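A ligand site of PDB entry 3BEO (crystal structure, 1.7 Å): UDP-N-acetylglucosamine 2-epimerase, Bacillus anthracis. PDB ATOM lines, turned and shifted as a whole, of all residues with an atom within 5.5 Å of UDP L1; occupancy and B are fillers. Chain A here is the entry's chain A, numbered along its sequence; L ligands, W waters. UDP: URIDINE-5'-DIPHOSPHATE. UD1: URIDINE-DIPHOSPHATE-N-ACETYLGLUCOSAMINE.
OG of Ser 290 is in hydrogen-bond range of N of Val 293 (3.2 Å).
OD1 of Asp 289 is in hydrogen-bond range of N of His 213 (2.9 Å).
The side-chain hydroxyl (OG) of Ser 290 sits at hydrogen-bond distance from the backbone NH (N) of Gly 292.
OE2 of Glu 296 sits at hydrogen-bond distance from NE2 of His 277 (2.9 Å).
N of Arg 214 sits at hydrogen-bond distance from OD2 of Asp 289, at 2.9 Å.
O2B of UD1 L2 sits at hydrogen-bond distance from NE2 of His 246, 2.9 Å away.
An oxygen (O3B) of UDP L1 sits at hydrogen-bond distance from the backbone NH of Gly 292 (2.9 Å).
O2' of UDP L1 lies within hydrogen-bond range of NE2 of His 277, at 3.1 Å.
O2A of UDP L1 lies within hydrogen-bond range of OG of Ser 290.
The backbone carbonyl oxygen of Leu 271 lies within hydrogen-bond range of a nitrogen (N3) of UDP L1 (2.7 Å).
The guanidinium group (NH2) of Arg 214 sits at hydrogen-bond distance from an oxygen (O4') of UD1 L2, 2.8 Å away.
The guanidinium group (NH1) of Arg 214 lies within salt-bridge range of an oxygen (O1B) of UDP L1 (2.9 Å).
A ring nitrogen (NE2) of His 213 is in hydrogen-bond range of an oxygen (O2A) of UDP L1 (3.2 Å).
O1B of UDP L1 sits at hydrogen-bond distance from N of Gly 291 (2.9 Å).
O4 of UDP L1 is in hydrogen-bond range of N of Leu 271 (3.1 Å).
The side-chain carboxylate of Glu 296 lies within hydrogen-bond range of an oxygen (O3') of UDP L1 (2.6 Å).
The guanidinium group (NH2) of Arg 18 is in salt-bridge range of an oxygen (O1A) of UDP L1 (2.9 Å).
Water W1 lies within hydrogen-bond range of O2A of UDP L1 (2.7 Å) and OG1 of Thr 211 (3.0 Å).
Water W2 lies within hydrogen-bond range of an oxygen (O3B) of UDP L1, the side-chain amino group (NZ) of Lys 23 and the backbone NH (N) of Gly 292.
Water W5 bridges O2 of UDP L1 and N of Val 273.
Water W4 lies within hydrogen-bond range of O of Pro 244 (2.8 Å), NH1 of Arg 18 (2.9 Å) and O4 of UDP L1 (3.0 Å).
Water W6 bridges the backbone carbonyl oxygen of Pro 19 and an oxygen (O3') of UDP L1.
Pro 19 touches UDP L1.
CD1 of Ile 22 touches O4' of UDP L1, 3.2 Å away.
Pro 244 touches UDP L1.
Pro 270 touches UDP L1.
Asp 272 touches UDP L1.
CA of Val 273 touches O2 of UDP L1, at 3.3 Å.
CD2 of Phe 276 touches O2' of UDP L1, at 3.3 Å.
Within 4 Å of UDP L1: Arg 18, Pro 19, Ile 22, His 213, Arg 214, Pro 244, Pro 270, Leu 271, Asp 272, Val 273, Phe 276, His 277, Ser 290, Gly 291, Gly 292 and Glu 296.
The nearest printed residue that does not touch UDP L1 is Val 293 (4.3 Å).
O2B of UDP L1 is in hydrogen-bond range of O4' of UD1 L2 (2.7 Å).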
ATOM      1  N   ARG A  18      -4.350 -17.448  19.497  1.00  0.00           N
ATOM      2  CA  ARG A  18      -3.299 -16.441  19.220  1.00  0.00           C
ATOM      3  C   ARG A  18      -3.179 -15.331  20.254  1.00  0.00           C
ATOM      4  O   ARG A  18      -2.058 -15.167  20.815  1.00  0.00           O
ATOM      5  CB  ARG A  18      -3.467 -15.831  17.834  1.00  0.00           C
ATOM      6  CG  ARG A  18      -2.572 -14.609  17.596  1.00  0.00           C
ATOM      7  CD  ARG A  18      -2.567 -14.147  16.158  1.00  0.00           C
ATOM      8  NE  ARG A  18      -3.838 -13.562  15.760  1.00  0.00           N
ATOM      9  CZ  ARG A  18      -4.163 -13.256  14.497  1.00  0.00           C
ATOM     10  NH1 ARG A  18      -3.333 -13.526  13.493  1.00  0.00           N
ATOM     11  NH2 ARG A  18      -5.358 -12.699  14.230  1.00  0.00           N
ATOM     12  N   PRO A  19      -4.271 -14.574  20.552  1.00  0.00           N
ATOM     13  CA  PRO A  19      -4.083 -13.437  21.450  1.00  0.00           C
ATOM     14  C   PRO A  19      -3.722 -13.835  22.867  1.00  0.00           C
ATOM     15  O   PRO A  19      -2.886 -13.169  23.505  1.00  0.00           O
ATOM     16  CB  PRO A  19      -5.446 -12.715  21.437  1.00  0.00           C
ATOM     17  CG  PRO A  19      -6.386 -13.753  20.942  1.00  0.00           C
ATOM     18  CD  PRO A  19      -5.638 -14.625  20.039  1.00  0.00           C
ATOM     19  N   ILE A  22       0.035 -14.786  22.918  1.00  0.00           N
ATOM     20  CA  ILE A  22       0.965 -13.639  22.904  1.00  0.00           C
ATOM     21  C   ILE A  22       1.061 -12.954  24.292  1.00  0.00           C
ATOM     22  O   ILE A  22       2.148 -12.624  24.768  1.00  0.00           O
ATOM     23  CB  ILE A  22       0.564 -12.630  21.829  1.00  0.00           C
ATOM     24  CG1 ILE A  22       0.751 -13.257  20.422  1.00  0.00           C
ATOM     25  CG2 ILE A  22       1.349 -11.291  22.008  1.00  0.00           C
ATOM     26  CD1 ILE A  22       0.074 -12.503  19.247  1.00  0.00           C
ATOM     27  N   LYS A  23      -0.063 -12.849  24.948  1.00  0.00           N
ATOM     28  CA  LYS A  23      -0.173 -12.163  26.242  1.00  0.00           C
ATOM     29  C   LYS A  23       0.291 -13.030  27.417  1.00  0.00           C
ATOM     30  O   LYS A  23       0.695 -12.490  28.465  1.00  0.00           O
ATOM     31  CB  LYS A  23      -1.578 -11.597  26.446  1.00  0.00           C
ATOM     32  CG  LYS A  23      -1.878 -10.343  25.629  1.00  0.00           C
ATOM     33  CD  LYS A  23      -3.334  -9.913  25.786  1.00  0.00           C
ATOM     34  CE  LYS A  23      -3.598  -8.457  25.294  1.00  0.00           C
ATOM     35  NZ  LYS A  23      -5.068  -8.135  25.202  1.00  0.00           N
ATOM     36  N   ASP A 104     -10.571 -13.284  27.937  1.00  0.00           N
ATOM     37  CA  ASP A 104     -12.016 -13.427  27.649  1.00  0.00           C
ATOM     38  C   ASP A 104     -12.455 -14.360  26.532  1.00  0.00           C
ATOM     39  O   ASP A 104     -13.519 -14.122  25.931  1.00  0.00           O
ATOM     40  CB  ASP A 104     -12.606 -12.029  27.464  1.00  0.00           C
ATOM     41  CG  ASP A 104     -11.891 -11.213  26.396  1.00  0.00           C
ATOM     42  OD1 ASP A 104     -11.457 -11.841  25.415  1.00  0.00           O
ATOM     43  OD2 ASP A 104     -11.807  -9.931  26.545  1.00  0.00           O
ATOM     44  N   THR A 211      -7.060  -5.357  10.388  1.00  0.00           N
ATOM     45  CA  THR A 211      -7.504  -6.704  10.785  1.00  0.00           C
ATOM     46  C   THR A 211      -8.991  -6.632  11.182  1.00  0.00           C
ATOM     47  O   THR A 211      -9.479  -5.598  11.682  1.00  0.00           O
ATOM     48  CB  THR A 211      -6.630  -7.286  11.944  1.00  0.00           C
ATOM     49  OG1 THR A 211      -6.981  -6.664  13.191  1.00  0.00           O
ATOM     50  CG2 THR A 211      -5.087  -7.111  11.664  1.00  0.00           C
ATOM     51  N   HIS A 213     -12.177  -9.468  12.654  1.00  0.00           N
ATOM     52  CA  HIS A 213     -12.643 -10.818  12.997  1.00  0.00           C
ATOM     53  C   HIS A 213     -13.690 -10.936  14.143  1.00  0.00           C
ATOM     54  O   HIS A 213     -14.029 -12.051  14.552  1.00  0.00           O
ATOM     55  CB  HIS A 213     -11.420 -11.727  13.365  1.00  0.00           C
ATOM     56  CG  HIS A 213     -10.747 -11.349  14.661  1.00  0.00           C
ATOM     57  ND1 HIS A 213     -11.064 -11.921  15.875  1.00  0.00           N
ATOM     58  CD2 HIS A 213      -9.761 -10.462  14.906  1.00  0.00           C
ATOM     59  CE1 HIS A 213     -10.295 -11.387  16.822  1.00  0.00           C
ATOM     60  NE2 HIS A 213      -9.485 -10.508  16.257  1.00  0.00           N
ATOM     61  N   ARG A 214     -14.157  -9.820  14.722  1.00  0.00           N
ATOM     62  CA  ARG A 214     -15.088  -9.911  15.852  1.00  0.00           C
ATOM     63  C   ARG A 214     -16.322 -10.680  15.394  1.00  0.00           C
ATOM     64  O   ARG A 214     -16.807 -10.484  14.244  1.00  0.00           O
ATOM     65  CB  ARG A 214     -15.514  -8.523  16.368  1.00  0.00           C
ATOM     66  CG  ARG A 214     -14.457  -7.743  17.067  1.00  0.00           C
ATOM     67  CD  ARG A 214     -14.455  -7.893  18.590  1.00  0.00           C
ATOM     68  NE  ARG A 214     -14.120  -9.257  19.012  1.00  0.00           N
ATOM     69  CZ  ARG A 214     -12.878  -9.734  19.112  1.00  0.00           C
ATOM     70  NH1 ARG A 214     -11.818  -8.973  18.855  1.00  0.00           N
ATOM     71  NH2 ARG A 214     -12.693 -11.002  19.499  1.00  0.00           N
ATOM     72  N   PRO A 244      -3.749  -8.922   7.018  1.00  0.00           N
ATOM     73  CA  PRO A 244      -3.477 -10.314   7.385  1.00  0.00           C
ATOM     74  C   PRO A 244      -4.819 -10.908   7.848  1.00  0.00           C
ATOM     75  O   PRO A 244      -5.266 -10.652   8.979  1.00  0.00           O
ATOM     76  CB  PRO A 244      -2.426 -10.176   8.525  1.00  0.00           C
ATOM     77  CG  PRO A 244      -1.986  -8.711   8.474  1.00  0.00           C
ATOM     78  CD  PRO A 244      -3.256  -8.021   8.056  1.00  0.00           C
ATOM     79  N   HIS A 246      -7.647 -13.155   9.202  1.00  0.00           N
ATOM     80  CA  HIS A 246      -7.948 -14.226  10.197  1.00  0.00           C
ATOM     81  C   HIS A 246      -8.362 -15.553   9.501  1.00  0.00           C
ATOM     82  O   HIS A 246      -8.971 -15.512   8.406  1.00  0.00           O
ATOM     83  CB  HIS A 246      -9.027 -13.695  11.101  1.00  0.00           C
ATOM     84  CG  HIS A 246      -9.339 -14.545  12.289  1.00  0.00           C
ATOM     85  ND1 HIS A 246      -9.857 -15.811  12.181  1.00  0.00           N
ATOM     86  CD2 HIS A 246      -9.183 -14.304  13.622  1.00  0.00           C
ATOM     87  CE1 HIS A 246     -10.058 -16.300  13.401  1.00  0.00           C
ATOM     88  NE2 HIS A 246      -9.641 -15.418  14.291  1.00  0.00           N
ATOM     89  N   GLU A 269      -1.714 -14.014   4.498  1.00  0.00           N
ATOM     90  CA  GLU A 269      -1.897 -14.928   5.628  1.00  0.00           C
ATOM     91  C   GLU A 269      -1.536 -14.208   6.919  1.00  0.00           C
ATOM     92  O   GLU A 269      -0.809 -13.247   6.888  1.00  0.00           O
ATOM     93  CB  GLU A 269      -1.037 -16.182   5.461  1.00  0.00           C
ATOM     94  CG  GLU A 269      -1.501 -17.116   4.362  1.00  0.00           C
ATOM     95  CD  GLU A 269      -2.856 -17.726   4.620  1.00  0.00           C
ATOM     96  OE1 GLU A 269      -3.160 -18.141   5.767  1.00  0.00           O
ATOM     97  OE2 GLU A 269      -3.648 -17.750   3.658  1.00  0.00           O
ATOM     98  N   PRO A 270      -2.070 -14.674   8.077  1.00  0.00           N
ATOM     99  CA  PRO A 270      -1.658 -14.124   9.360  1.00  0.00           C
ATOM    100  C   PRO A 270      -0.153 -14.005   9.539  1.00  0.00           C
ATOM    101  O   PRO A 270       0.589 -14.937   9.196  1.00  0.00           O
ATOM    102  CB  PRO A 270      -2.230 -15.126  10.358  1.00  0.00           C
ATOM    103  CG  PRO A 270      -3.484 -15.617   9.673  1.00  0.00           C
ATOM    104  CD  PRO A 270      -3.166 -15.654   8.228  1.00  0.00           C
ATOM    105  N   LEU A 271       0.283 -12.838   9.998  1.00  0.00           N
ATOM    106  CA  LEU A 271       1.715 -12.581  10.233  1.00  0.00           C
ATOM    107  C   LEU A 271       2.096 -13.094  11.608  1.00  0.00           C
ATOM    108  O   LEU A 271       1.271 -13.083  12.538  1.00  0.00           O
ATOM    109  CB  LEU A 271       2.053 -11.094  10.137  1.00  0.00           C
ATOM    110  CG  LEU A 271       1.979 -10.475   8.742  1.00  0.00           C
ATOM    111  CD1 LEU A 271       2.110  -8.940   8.843  1.00  0.00           C
ATOM    112  CD2 LEU A 271       3.047 -11.071   7.868  1.00  0.00           C
ATOM    113  N   ASP A 272       3.322 -13.568  11.742  1.00  0.00           N
ATOM    114  CA  ASP A 272       3.771 -13.920  13.088  1.00  0.00           C
ATOM    115  C   ASP A 272       3.891 -12.629  13.921  1.00  0.00           C
ATOM    116  O   ASP A 272       3.848 -11.534  13.365  1.00  0.00           O
ATOM    117  CB  ASP A 272       5.019 -14.807  13.056  1.00  0.00           C
ATOM    118  CG  ASP A 272       6.314 -14.058  12.738  1.00  0.00           C
ATOM    119  OD1 ASP A 272       6.537 -12.940  13.225  1.00  0.00           O
ATOM    120  OD2 ASP A 272       7.176 -14.654  12.043  1.00  0.00           O
ATOM    121  N   VAL A 273       3.974 -12.725  15.245  1.00  0.00           N
ATOM    122  CA  VAL A 273       3.892 -11.541  16.085  1.00  0.00           C
ATOM    123  C   VAL A 273       5.088 -10.577  15.889  1.00  0.00           C
ATOM    124  O   VAL A 273       4.907  -9.359  16.010  1.00  0.00           O
ATOM    125  CB  VAL A 273       3.705 -11.936  17.594  1.00  0.00           C
ATOM    126  CG1 VAL A 273       4.980 -12.582  18.112  1.00  0.00           C
ATOM    127  CG2 VAL A 273       3.229 -10.717  18.426  1.00  0.00           C
ATOM    128  N   PHE A 276       4.140  -8.781  12.624  1.00  0.00           N
ATOM    129  CA  PHE A 276       3.014  -7.931  12.805  1.00  0.00           C
ATOM    130  C   PHE A 276       3.346  -6.688  13.633  1.00  0.00           C
ATOM    131  O   PHE A 276       2.996  -5.591  13.247  1.00  0.00           O
ATOM    132  CB  PHE A 276       1.818  -8.668  13.417  1.00  0.00           C
ATOM    133  CG  PHE A 276       0.588  -7.843  13.438  1.00  0.00           C
ATOM    134  CD1 PHE A 276      -0.266  -7.819  12.336  1.00  0.00           C
ATOM    135  CD2 PHE A 276       0.303  -7.003  14.523  1.00  0.00           C
ATOM    136  CE1 PHE A 276      -1.429  -7.061  12.355  1.00  0.00           C
ATOM    137  CE2 PHE A 276      -0.826  -6.214  14.534  1.00  0.00           C
ATOM    138  CZ  PHE A 276      -1.697  -6.250  13.451  1.00  0.00           C
ATOM    139  N   HIS A 277       3.962  -6.858  14.807  1.00  0.00           N
ATOM    140  CA  HIS A 277       4.330  -5.710  15.621  1.00  0.00           C
ATOM    141  C   HIS A 277       5.213  -4.706  14.874  1.00  0.00           C
ATOM    142  O   HIS A 277       4.979  -3.508  14.947  1.00  0.00           O
ATOM    143  CB  HIS A 277       5.057  -6.131  16.869  1.00  0.00           C
ATOM    144  CG  HIS A 277       4.141  -6.722  17.898  1.00  0.00           C
ATOM    145  ND1 HIS A 277       4.599  -7.351  19.028  1.00  0.00           N
ATOM    146  CD2 HIS A 277       2.780  -6.740  17.970  1.00  0.00           C
ATOM    147  CE1 HIS A 277       3.568  -7.717  19.774  1.00  0.00           C
ATOM    148  NE2 HIS A 277       2.456  -7.380  19.140  1.00  0.00           N
ATOM    149  N   ASP A 289     -10.759  -4.302  14.613  1.00  0.00           N
ATOM    150  CA  ASP A 289     -11.668  -4.655  15.694  1.00  0.00           C
ATOM    151  C   ASP A 289     -10.985  -5.649  16.687  1.00  0.00           C
ATOM    152  O   ASP A 289     -11.626  -6.253  17.544  1.00  0.00           O
ATOM    153  CB  ASP A 289     -13.029  -5.153  15.147  1.00  0.00           C
ATOM    154  CG  ASP A 289     -12.942  -6.520  14.435  1.00  0.00           C
ATOM    155  OD1 ASP A 289     -11.890  -7.175  14.393  1.00  0.00           O
ATOM    156  OD2 ASP A 289     -14.010  -7.013  13.958  1.00  0.00           O
ATOM    157  N   SER A 290      -9.643  -5.673  16.646  1.00  0.00           N
ATOM    158  CA  SER A 290      -8.819  -6.517  17.536  1.00  0.00           C
ATOM    159  C   SER A 290      -8.678  -5.859  18.894  1.00  0.00           C
ATOM    160  O   SER A 290      -8.481  -4.657  19.009  1.00  0.00           O
ATOM    161  CB  SER A 290      -7.405  -6.733  16.927  1.00  0.00           C
ATOM    162  OG  SER A 290      -6.428  -7.110  17.888  1.00  0.00           O
ATOM    163  N   GLY A 291      -8.697  -6.672  19.945  1.00  0.00           N
ATOM    164  CA  GLY A 291      -8.455  -6.164  21.306  1.00  0.00           C
ATOM    165  C   GLY A 291      -6.984  -5.827  21.528  1.00  0.00           C
ATOM    166  O   GLY A 291      -6.647  -4.741  21.998  1.00  0.00           O
ATOM    167  N   GLY A 292      -6.110  -6.775  21.241  1.00  0.00           N
ATOM    168  CA  GLY A 292      -4.689  -6.558  21.522  1.00  0.00           C
ATOM    169  C   GLY A 292      -4.069  -5.370  20.780  1.00  0.00           C
ATOM    170  O   GLY A 292      -3.156  -4.708  21.277  1.00  0.00           O
ATOM    171  N   VAL A 293      -4.487  -5.164  19.542  1.00  0.00           N
ATOM    172  CA  VAL A 293      -3.951  -4.033  18.734  1.00  0.00           C
ATOM    173  C   VAL A 293      -4.263  -2.686  19.443  1.00  0.00           C
ATOM    174  O   VAL A 293      -3.411  -1.765  19.547  1.00  0.00           O
ATOM    175  CB  VAL A 293      -4.525  -4.064  17.315  1.00  0.00           C
ATOM    176  CG1 VAL A 293      -4.205  -2.822  16.562  1.00  0.00           C
ATOM    177  CG2 VAL A 293      -4.041  -5.333  16.586  1.00  0.00           C
ATOM    178  N   GLU A 296      -1.592  -2.205  22.099  1.00  0.00           N
ATOM    179  CA  GLU A 296      -0.226  -2.041  21.556  1.00  0.00           C
ATOM    180  C   GLU A 296      -0.028  -0.672  20.853  1.00  0.00           C
ATOM    181  O   GLU A 296       1.015  -0.041  20.965  1.00  0.00           O
ATOM    182  CB  GLU A 296       0.042  -3.172  20.563  1.00  0.00           C
ATOM    183  CG  GLU A 296       0.100  -4.563  21.204  1.00  0.00           C
ATOM    184  CD  GLU A 296      -0.127  -5.705  20.234  1.00  0.00           C
ATOM    185  OE1 GLU A 296      -0.467  -5.449  19.034  1.00  0.00           O
ATOM    186  OE2 GLU A 296       0.082  -6.856  20.700  1.00  0.00           O
HETATM  187  N1  UDP L   1      -1.343 -10.283  15.597  1.00  0.00           N
HETATM  188  C2  UDP L   1      -0.337 -10.974  14.973  1.00  0.00           C
HETATM  189  N3  UDP L   1      -0.431 -11.266  13.612  1.00  0.00           N
HETATM  190  C4  UDP L   1      -1.546 -10.872  12.904  1.00  0.00           C
HETATM  191  C5  UDP L   1      -2.573 -10.176  13.539  1.00  0.00           C
HETATM  192  C6  UDP L   1      -2.449  -9.873  14.902  1.00  0.00           C
HETATM  193  O2  UDP L   1       0.668 -11.356  15.615  1.00  0.00           O
HETATM  194  O4  UDP L   1      -1.587 -11.123  11.712  1.00  0.00           O
HETATM  195  C1' UDP L   1      -1.261 -10.041  17.057  1.00  0.00           C
HETATM  196  C2' UDP L   1      -1.497  -8.638  17.602  1.00  0.00           C
HETATM  197  O2' UDP L   1      -0.299  -7.875  17.701  1.00  0.00           O
HETATM  198  C3' UDP L   1      -2.024  -8.954  18.997  1.00  0.00           C
HETATM  199  C4' UDP L   1      -2.759 -10.275  18.830  1.00  0.00           C
HETATM  200  O4' UDP L   1      -2.222 -10.920  17.671  1.00  0.00           O
HETATM  201  O3' UDP L   1      -1.006  -9.103  19.989  1.00  0.00           O
HETATM  202  C5' UDP L   1      -4.220  -9.968  18.743  1.00  0.00           C
HETATM  203  O5' UDP L   1      -4.868 -11.115  18.391  1.00  0.00           O
HETATM  204  PA  UDP L   1      -6.336 -11.050  17.699  1.00  0.00           P
HETATM  205  O1A UDP L   1      -6.405 -12.291  16.884  1.00  0.00           O
HETATM  206  O2A UDP L   1      -6.522  -9.712  17.020  1.00  0.00           O
HETATM  207  O3A UDP L   1      -7.417 -11.299  18.865  1.00  0.00           O
HETATM  208  PB  UDP L   1      -7.993 -10.306  19.930  1.00  0.00           P
HETATM  209  O1B UDP L   1      -8.986  -9.439  19.241  1.00  0.00           O
HETATM  210  O2B UDP L   1      -8.515 -11.212  21.023  1.00  0.00           O
HETATM  211  O3B UDP L   1      -6.931  -9.441  20.526  1.00  0.00           O
HETATM  212  C1' UD1 L   2     -11.498 -16.483  18.879  1.00  0.00           C
HETATM  213  C2' UD1 L   2     -12.001 -15.888  20.218  1.00  0.00           C
HETATM  214  C3' UD1 L   2     -11.860 -14.375  20.260  1.00  0.00           C
HETATM  215  C4' UD1 L   2     -10.454 -13.958  19.822  1.00  0.00           C
HETATM  216  C5' UD1 L   2     -10.001 -14.633  18.554  1.00  0.00           C
HETATM  217  C6' UD1 L   2      -8.519 -14.337  18.263  1.00  0.00           C
HETATM  218  C7' UD1 L   2     -13.808 -16.924  21.534  1.00  0.00           C
HETATM  219  C8' UD1 L   2     -15.280 -16.912  21.838  1.00  0.00           C
HETATM  220  N2' UD1 L   2     -13.375 -16.222  20.463  1.00  0.00           N
HETATM  221  O1' UD1 L   2     -12.395 -16.119  17.868  1.00  0.00           O
HETATM  222  O3' UD1 L   2     -12.089 -13.860  21.576  1.00  0.00           O
HETATM  223  O4' UD1 L   2     -10.370 -12.543  19.635  1.00  0.00           O
HETATM  224  O5' UD1 L   2     -10.202 -16.048  18.655  1.00  0.00           O
HETATM  225  O6' UD1 L   2      -8.191 -14.540  16.862  1.00  0.00           O
HETATM  226  O7' UD1 L   2     -13.090 -17.489  22.285  1.00  0.00           O
HETATM  227  N1  UD1 L   2      -9.404 -21.264  12.544  1.00  0.00           N
HETATM  228  C2  UD1 L   2      -8.394 -21.962  11.893  1.00  0.00           C
HETATM  229  N3  UD1 L   2      -7.129 -21.940  12.388  1.00  0.00           N
HETATM  230  C4  UD1 L   2      -6.842 -21.265  13.515  1.00  0.00           C
HETATM  231  C5  UD1 L   2      -7.808 -20.511  14.116  1.00  0.00           C
HETATM  232  C6  UD1 L   2      -9.087 -20.534  13.640  1.00  0.00           C
HETATM  233  O2  UD1 L   2      -8.670 -22.651  10.867  1.00  0.00           O
HETATM  234  O4  UD1 L   2      -5.678 -21.255  14.004  1.00  0.00           O
HETATM  235  C1B UD1 L   2     -10.778 -21.283  11.978  1.00  0.00           C
HETATM  236  C2B UD1 L   2     -11.454 -22.658  12.233  1.00  0.00           C
HETATM  237  O2' UD1 L   2     -12.390 -22.976  11.225  1.00  0.00           O
HETATM  238  C3B UD1 L   2     -12.151 -22.476  13.585  1.00  0.00           C
HETATM  239  C4B UD1 L   2     -12.155 -20.970  13.685  1.00  0.00           C
HETATM  240  O4B UD1 L   2     -11.583 -20.285  12.574  1.00  0.00           O
HETATM  241  O3B UD1 L   2     -13.366 -23.208  13.860  1.00  0.00           O
HETATM  242  C5B UD1 L   2     -13.176 -20.159  14.439  1.00  0.00           C
HETATM  243  O5B UD1 L   2     -12.200 -20.123  15.511  1.00  0.00           O
HETATM  244  PA  UD1 L   2     -12.720 -19.688  16.939  1.00  0.00           P
HETATM  245  O1A UD1 L   2     -13.900 -20.559  17.137  1.00  0.00           O
HETATM  246  O2A UD1 L   2     -11.486 -19.715  17.803  1.00  0.00           O
HETATM  247  O3A UD1 L   2     -13.214 -18.180  16.771  1.00  0.00           O
HETATM  248  PB  UD1 L   2     -12.352 -16.873  16.469  1.00  0.00           P
HETATM  249  O1B UD1 L   2     -13.284 -16.009  15.615  1.00  0.00           O
HETATM  250  O2B UD1 L   2     -10.958 -17.233  16.078  1.00  0.00           O
HETATM  251  O   HOH W   1      -5.739  -9.112  14.519  1.00  0.00           O
HETATM  252  O   HOH W   2      -5.503  -9.668  22.796  1.00  0.00           O
HETATM  253  O   HOH W   3      -7.510 -11.214  24.111  1.00  0.00           O
HETATM  254  O   HOH W   4      -4.383 -11.989  11.231  1.00  0.00           O
HETATM  255  O   HOH W   5       1.055 -14.273  15.823  1.00  0.00           O
HETATM  256  O   HOH W   6      -2.752 -10.507  22.266  1.00  0.00           O
